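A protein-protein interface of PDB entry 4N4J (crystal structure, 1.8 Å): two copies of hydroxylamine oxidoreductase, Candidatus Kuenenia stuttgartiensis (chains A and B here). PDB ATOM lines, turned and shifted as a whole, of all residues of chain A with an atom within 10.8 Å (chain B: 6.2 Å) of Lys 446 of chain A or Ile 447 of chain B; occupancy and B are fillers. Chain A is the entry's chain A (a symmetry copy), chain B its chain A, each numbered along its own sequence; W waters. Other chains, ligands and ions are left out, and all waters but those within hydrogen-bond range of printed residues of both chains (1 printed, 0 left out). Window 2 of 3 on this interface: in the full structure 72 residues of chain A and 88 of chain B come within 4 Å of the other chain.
N of Leu 449 of chain B is in hydrogen-bond range of O of Glu 444 of chain B, 2.9 Å away.
Ala 442 of chain A touches Leu 449 of chain B, but with the chains exchanged Leu 449 of chain A does not touch Ala 442 of chain B (13.4 Å).
Ile 443 of chain A touches Glu 444 of chain B, but with the chains exchanged Glu 444 of chain A does not touch Ile 443 of chain B (7.0 Å).
Ile 443 of chain A touches Leu 449 of chain B, but with the chains exchanged Leu 449 of chain A does not touch Ile 443 of chain B (8.9 Å).
Lys 446 of chain A touches Ile 447 of chain B, but with the chains exchanged Ile 447 of chain A does not touch Lys 446 of chain B (7.6 Å).
Positions printed for both chains: 442, 443, 444, 445, 446, 447, 448 and 449.
Water W1 lies within hydrogen-bond range of OE1 of Glu 444 of chain B (2.7 Å) and O of Arg 439 of chain A (2.8 Å).
Among the printed residues, pairs that only touch across the chains: Lys 446 of chain A with Ile 447 of chain B, Ala 442 of chain A with Leu 449 of chain B, Ile 443 of chain A with Ile 443 of chain B, Ile 447 of chain A with Ile 447 of chain B, Ile 443 of chain A with Leu 449 of chain B, Lys 446 of chain A with Leu 449 of chain B, Lys 446 of chain A with Gly 448 of chain B and Ile 443 of chain A with Glu 444 of chain B.
The guanidinium group of Arg 439 of chain A is in salt-bridge range of the side-chain carboxylate of Glu 444 of chain B (2.8 Å).
Hydrophobic or aromatic side chains of chain B within 4 Å of the printed part of chain A: Ile 443, Ile 447 and Leu 449.
Hydrophobic or aromatic side chains of chain A that line the printed part of chain B: Ile 443 and Ile 447.
Among the printed residues, Asp or Glu carboxylates within 4 Å of a Lys or Arg side-chain nitrogen of the other chain: Arg 439 of chain A with Glu 444 of chain B (2.8 Å).
Lys 446 of chain A touches three residues of chain B.
Of the printed residues of chain A, Ile 447 of chain B touches Lys 446 and Ile 447.
No residue of chain A comes within 4 Å of Lys 446 of chain B.
Of the printed residues of chain A, Gly 448 of chain B touches Lys 446 (3.9 Å).
Of the printed residues of chain A, Leu 449 of chain B touches Ala 442, Ile 443 and Lys 446.
Printed residues of chain B within 4 Å of Arg 439 of chain A: Glu 444.
Of the printed residues of chain B, Ala 442 of chain A touches Leu 449 (3.6 Å).
The nearest printed residue of chain B that does not touch Lys 446 of chain A is Glu 444 of chain B (6.5 Å).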
ATOM      1  N   ARG A 438     -20.137   1.821  24.662  1.00  0.00           N
ATOM      2  CA  ARG A 438     -19.433   2.387  23.516  1.00  0.00           C
ATOM      3  C   ARG A 438     -20.324   3.307  22.680  1.00  0.00           C
ATOM      4  O   ARG A 438     -19.867   4.364  22.227  1.00  0.00           O
ATOM      5  CB  ARG A 438     -18.807   1.275  22.672  1.00  0.00           C
ATOM      6  CG  ARG A 438     -17.623   0.638  23.382  1.00  0.00           C
ATOM      7  CD  ARG A 438     -16.984  -0.482  22.587  1.00  0.00           C
ATOM      8  NE  ARG A 438     -15.824  -1.019  23.295  1.00  0.00           N
ATOM      9  CZ  ARG A 438     -14.635  -0.420  23.370  1.00  0.00           C
ATOM     10  NH1 ARG A 438     -14.418   0.752  22.769  1.00  0.00           N
ATOM     11  NH2 ARG A 438     -13.652  -0.996  24.047  1.00  0.00           N
ATOM     12  N   ARG A 439     -21.592   2.936  22.505  1.00  0.00           N
ATOM     13  CA  ARG A 439     -22.530   3.772  21.753  1.00  0.00           C
ATOM     14  C   ARG A 439     -22.830   5.088  22.457  1.00  0.00           C
ATOM     15  O   ARG A 439     -22.886   6.134  21.807  1.00  0.00           O
ATOM     16  CB  ARG A 439     -23.836   3.037  21.468  1.00  0.00           C
ATOM     17  CG  ARG A 439     -23.704   1.967  20.413  1.00  0.00           C
ATOM     18  CD  ARG A 439     -25.019   1.247  20.175  1.00  0.00           C
ATOM     19  NE  ARG A 439     -25.789   1.817  19.072  1.00  0.00           N
ATOM     20  CZ  ARG A 439     -26.906   1.279  18.588  1.00  0.00           C
ATOM     21  NH1 ARG A 439     -27.405   0.166  19.119  1.00  0.00           N
ATOM     22  NH2 ARG A 439     -27.536   1.855  17.574  1.00  0.00           N
ATOM     23  N   PHE A 440     -23.030   5.038  23.774  1.00  0.00           N
ATOM     24  CA  PHE A 440     -23.227   6.259  24.556  1.00  0.00           C
ATOM     25  C   PHE A 440     -22.020   7.186  24.445  1.00  0.00           C
ATOM     26  O   PHE A 440     -22.176   8.385  24.195  1.00  0.00           O
ATOM     27  CB  PHE A 440     -23.466   5.955  26.041  1.00  0.00           C
ATOM     28  CG  PHE A 440     -24.911   5.734  26.406  1.00  0.00           C
ATOM     29  CD1 PHE A 440     -25.897   6.634  26.014  1.00  0.00           C
ATOM     30  CD2 PHE A 440     -25.279   4.645  27.187  1.00  0.00           C
ATOM     31  CE1 PHE A 440     -27.224   6.435  26.367  1.00  0.00           C
ATOM     32  CE2 PHE A 440     -26.603   4.440  27.543  1.00  0.00           C
ATOM     33  CZ  PHE A 440     -27.580   5.332  27.132  1.00  0.00           C
ATOM     34  N   ALA A 441     -20.830   6.629  24.652  1.00  0.00           N
ATOM     35  CA  ALA A 441     -19.592   7.409  24.607  1.00  0.00           C
ATOM     36  C   ALA A 441     -19.373   8.041  23.234  1.00  0.00           C
ATOM     37  O   ALA A 441     -18.958   9.197  23.143  1.00  0.00           O
ATOM     38  CB  ALA A 441     -18.395   6.536  24.986  1.00  0.00           C
ATOM     39  N   ALA A 442     -19.651   7.282  22.176  1.00  0.00           N
ATOM     40  CA  ALA A 442     -19.510   7.773  20.800  1.00  0.00           C
ATOM     41  C   ALA A 442     -20.460   8.940  20.521  1.00  0.00           C
ATOM     42  O   ALA A 442     -20.067   9.942  19.913  1.00  0.00           O
ATOM     43  CB  ALA A 442     -19.754   6.647  19.808  1.00  0.00           C
ATOM     44  N   ILE A 443     -21.705   8.807  20.973  1.00  0.00           N
ATOM     45  CA  ILE A 443     -22.715   9.853  20.808  1.00  0.00           C
ATOM     46  C   ILE A 443     -22.326  11.099  21.597  1.00  0.00           C
ATOM     47  O   ILE A 443     -22.316  12.207  21.062  1.00  0.00           O
ATOM     48  CB  ILE A 443     -24.110   9.377  21.276  1.00  0.00           C
ATOM     49  CG1 ILE A 443     -24.697   8.391  20.262  1.00  0.00           C
ATOM     50  CG2 ILE A 443     -25.057  10.564  21.465  1.00  0.00           C
ATOM     51  CD1 ILE A 443     -25.797   7.508  20.822  1.00  0.00           C
ATOM     52  N   GLU A 444     -21.992  10.905  22.867  1.00  0.00           N
ATOM     53  CA  GLU A 444     -21.632  12.017  23.742  1.00  0.00           C
ATOM     54  C   GLU A 444     -20.402  12.778  23.244  1.00  0.00           C
ATOM     55  O   GLU A 444     -20.351  14.010  23.329  1.00  0.00           O
ATOM     56  CB  GLU A 444     -21.431  11.515  25.170  1.00  0.00           C
ATOM     57  CG  GLU A 444     -22.748  11.096  25.821  1.00  0.00           C
ATOM     58  CD  GLU A 444     -22.581  10.191  27.027  1.00  0.00           C
ATOM     59  OE1 GLU A 444     -23.611   9.855  27.647  1.00  0.00           O
ATOM     60  OE2 GLU A 444     -21.440   9.810  27.355  1.00  0.00           O
ATOM     61  N   LYS A 445     -19.422  12.047  22.719  1.00  0.00           N
ATOM     62  CA  LYS A 445     -18.242  12.663  22.127  1.00  0.00           C
ATOM     63  C   LYS A 445     -18.627  13.513  20.914  1.00  0.00           C
ATOM     64  O   LYS A 445     -18.190  14.658  20.794  1.00  0.00           O
ATOM     65  CB  LYS A 445     -17.221  11.597  21.720  1.00  0.00           C
ATOM     66  CG  LYS A 445     -15.993  12.155  21.003  1.00  0.00           C
ATOM     67  CD  LYS A 445     -14.839  11.162  20.998  1.00  0.00           C
ATOM     68  CE  LYS A 445     -13.612  11.755  20.318  1.00  0.00           C
ATOM     69  NZ  LYS A 445     -12.388  10.938  20.560  1.00  0.00           N
ATOM     70  N   LYS A 446     -19.449  12.960  20.027  1.00  0.00           N
ATOM     71  CA  LYS A 446     -19.815  13.668  18.799  1.00  0.00           C
ATOM     72  C   LYS A 446     -20.568  14.965  19.076  1.00  0.00           C
ATOM     73  O   LYS A 446     -20.303  15.985  18.435  1.00  0.00           O
ATOM     74  CB  LYS A 446     -20.644  12.785  17.866  1.00  0.00           C
ATOM     75  CG  LYS A 446     -20.895  13.439  16.513  1.00  0.00           C
ATOM     76  CD  LYS A 446     -21.635  12.532  15.560  1.00  0.00           C
ATOM     77  CE  LYS A 446     -21.896  13.243  14.238  1.00  0.00           C
ATOM     78  NZ  LYS A 446     -20.648  13.647  13.545  1.00  0.00           N
ATOM     79  N   ILE A 447     -21.502  14.929  20.024  1.00  0.00           N
ATOM     80  CA  ILE A 447     -22.326  16.106  20.327  1.00  0.00           C
ATOM     81  C   ILE A 447     -21.709  17.020  21.395  1.00  0.00           C
ATOM     82  O   ILE A 447     -22.300  18.037  21.754  1.00  0.00           O
ATOM     83  CB  ILE A 447     -23.767  15.708  20.739  1.00  0.00           C
ATOM     84  CG1 ILE A 447     -23.800  15.074  22.136  1.00  0.00           C
ATOM     85  CG2 ILE A 447     -24.371  14.773  19.698  1.00  0.00           C
ATOM     86  CD1 ILE A 447     -25.187  14.664  22.579  1.00  0.00           C
ATOM     87  N   GLY A 448     -20.535  16.653  21.903  1.00  0.00           N
ATOM     88  CA  GLY A 448     -19.842  17.464  22.899  1.00  0.00           C
ATOM     89  C   GLY A 448     -20.545  17.516  24.244  1.00  0.00           C
ATOM     90  O   GLY A 448     -20.497  18.536  24.934  1.00  0.00           O
ATOM     91  N   LEU A 449     -21.205  16.420  24.614  1.00  0.00           N
ATOM     92  CA  LEU A 449     -21.837  16.306  25.923  1.00  0.00           C
ATOM     93  C   LEU A 449     -20.820  15.703  26.883  1.00  0.00           C
ATOM     94  O   LEU A 449     -20.322  14.603  26.651  1.00  0.00           O
ATOM     95  CB  LEU A 449     -23.090  15.426  25.843  1.00  0.00           C
ATOM     96  CG  LEU A 449     -24.001  15.377  27.076  1.00  0.00           C
ATOM     97  CD1 LEU A 449     -25.394  14.898  26.691  1.00  0.00           C
ATOM     98  CD2 LEU A 449     -23.419  14.492  28.179  1.00  0.00           C
ATOM     99  N   GLU A 450     -20.499  16.432  27.949  1.00  0.00           N
ATOM    100  CA  GLU A 450     -19.564  15.939  28.955  1.00  0.00           C
ATOM    101  C   GLU A 450     -20.326  15.107  29.978  1.00  0.00           C
ATOM    102  O   GLU A 450     -20.946  15.646  30.898  1.00  0.00           O
ATOM    103  CB  GLU A 450     -18.833  17.095  29.643  1.00  0.00           C
ATOM    104  CG  GLU A 450     -17.782  16.635  30.657  1.00  0.00           C
ATOM    105  CD  GLU A 450     -16.848  17.752  31.105  1.00  0.00           C
ATOM    106  OE1 GLU A 450     -16.463  17.762  32.299  1.00  0.00           O
ATOM    107  OE2 GLU A 450     -16.494  18.616  30.266  1.00  0.00           O
ATOM    108  N   HIS A 451     -20.290  13.792  29.803  1.00  0.00           N
ATOM    109  CA  HIS A 451     -20.992  12.890  30.706  1.00  0.00           C
ATOM    110  C   HIS A 451     -20.189  12.681  31.979  1.00  0.00           C
ATOM    111  O   HIS A 451     -18.997  12.384  31.929  1.00  0.00           O
ATOM    112  CB  HIS A 451     -21.250  11.536  30.046  1.00  0.00           C
ATOM    113  CG  HIS A 451     -21.711  10.485  31.007  1.00  0.00           C
ATOM    114  ND1 HIS A 451     -22.977  10.481  31.551  1.00  0.00           N
ATOM    115  CD2 HIS A 451     -21.068   9.418  31.540  1.00  0.00           C
ATOM    116  CE1 HIS A 451     -23.098   9.449  32.368  1.00  0.00           C
ATOM    117  NE2 HIS A 451     -21.953   8.789  32.380  1.00  0.00           N
ATOM    118  N   ALA B 442     -32.382   6.228  16.850  1.00  0.00           N
ATOM    119  CA  ALA B 442     -33.019   7.535  16.642  1.00  0.00           C
ATOM    120  C   ALA B 442     -32.032   8.682  16.868  1.00  0.00           C
ATOM    121  O   ALA B 442     -31.988   9.639  16.087  1.00  0.00           O
ATOM    122  CB  ALA B 442     -34.224   7.687  17.556  1.00  0.00           C
ATOM    123  N   ILE B 443     -31.242   8.577  17.934  1.00  0.00           N
ATOM    124  CA  ILE B 443     -30.229   9.582  18.260  1.00  0.00           C
ATOM    125  C   ILE B 443     -29.147   9.617  17.186  1.00  0.00           C
ATOM    126  O   ILE B 443     -28.812  10.680  16.663  1.00  0.00           O
ATOM    127  CB  ILE B 443     -29.568   9.301  19.630  1.00  0.00           C
ATOM    128  CG1 ILE B 443     -30.539   9.641  20.763  1.00  0.00           C
ATOM    129  CG2 ILE B 443     -28.273  10.102  19.786  1.00  0.00           C
ATOM    130  CD1 ILE B 443     -30.208   8.973  22.085  1.00  0.00           C
ATOM    131  N   GLU B 444     -28.619   8.447  16.850  1.00  0.00           N
ATOM    132  CA  GLU B 444     -27.551   8.346  15.859  1.00  0.00           C
ATOM    133  C   GLU B 444     -27.979   8.862  14.484  1.00  0.00           C
ATOM    134  O   GLU B 444     -27.193   9.513  13.788  1.00  0.00           O
ATOM    135  CB  GLU B 444     -27.049   6.906  15.778  1.00  0.00           C
ATOM    136  CG  GLU B 444     -26.272   6.498  17.030  1.00  0.00           C
ATOM    137  CD  GLU B 444     -26.142   4.998  17.215  1.00  0.00           C
ATOM    138  OE1 GLU B 444     -25.470   4.590  18.184  1.00  0.00           O
ATOM    139  OE2 GLU B 444     -26.705   4.230  16.410  1.00  0.00           O
ATOM    140  N   LYS B 445     -29.222   8.578  14.103  1.00  0.00           N
ATOM    141  CA  LYS B 445     -29.774   9.092  12.857  1.00  0.00           C
ATOM    142  C   LYS B 445     -29.841  10.620  12.886  1.00  0.00           C
ATOM    143  O   LYS B 445     -29.421  11.279  11.933  1.00  0.00           O
ATOM    144  CB  LYS B 445     -31.167   8.510  12.601  1.00  0.00           C
ATOM    145  CG  LYS B 445     -31.858   9.073  11.360  1.00  0.00           C
ATOM    146  CD  LYS B 445     -33.013   8.192  10.905  1.00  0.00           C
ATOM    147  CE  LYS B 445     -33.659   8.748   9.642  1.00  0.00           C
ATOM    148  NZ  LYS B 445     -34.583   7.766   9.006  1.00  0.00           N
ATOM    149  N   LYS B 446     -30.356  11.181  13.976  1.00  0.00           N
ATOM    150  CA  LYS B 446     -30.527  12.632  14.065  1.00  0.00           C
ATOM    151  C   LYS B 446     -29.201  13.382  13.989  1.00  0.00           C
ATOM    152  O   LYS B 446     -29.107  14.408  13.311  1.00  0.00           O
ATOM    153  CB  LYS B 446     -31.270  13.035  15.339  1.00  0.00           C
ATOM    154  CG  LYS B 446     -31.608  14.520  15.373  1.00  0.00           C
ATOM    155  CD  LYS B 446     -32.421  14.900  16.588  1.00  0.00           C
ATOM    156  CE  LYS B 446     -32.700  16.398  16.598  1.00  0.00           C
ATOM    157  NZ  LYS B 446     -33.479  16.847  15.417  1.00  0.00           N
ATOM    158  N   ILE B 447     -28.182  12.877  14.681  1.00  0.00           N
ATOM    159  CA  ILE B 447     -26.881  13.554  14.726  1.00  0.00           C
ATOM    160  C   ILE B 447     -25.933  13.122  13.598  1.00  0.00           C
ATOM    161  O   ILE B 447     -24.803  13.602  13.522  1.00  0.00           O
ATOM    162  CB  ILE B 447     -26.185  13.373  16.100  1.00  0.00           C
ATOM    163  CG1 ILE B 447     -25.673  11.939  16.289  1.00  0.00           C
ATOM    164  CG2 ILE B 447     -27.135  13.769  17.225  1.00  0.00           C
ATOM    165  CD1 ILE B 447     -24.991  11.713  17.620  1.00  0.00           C
ATOM    166  N   GLY B 448     -26.389  12.215  12.737  1.00  0.00           N
ATOM    167  CA  GLY B 448     -25.586  11.757  11.607  1.00  0.00           C
ATOM    168  C   GLY B 448     -24.370  10.941  12.010  1.00  0.00           C
ATOM    169  O   GLY B 448     -23.330  11.006  11.352  1.00  0.00           O
ATOM    170  N   LEU B 449     -24.498  10.179  13.095  1.00  0.00           N
ATOM    171  CA  LEU B 449     -23.441   9.273  13.528  1.00  0.00           C
ATOM    172  C   LEU B 449     -23.681   7.922  12.867  1.00  0.00           C
ATOM    173  O   LEU B 449     -24.737   7.320  13.049  1.00  0.00           O
ATOM    174  CB  LEU B 449     -23.441   9.134  15.055  1.00  0.00           C
ATOM    175  CG  LEU B 449     -22.261   8.397  15.700  1.00  0.00           C
ATOM    176  CD1 LEU B 449     -22.143   8.764  17.172  1.00  0.00           C
ATOM    177  CD2 LEU B 449     -22.379   6.880  15.536  1.00  0.00           C
HETATM  178  O   HOH W   1     -23.135   5.560  19.082  1.00  0.00           O
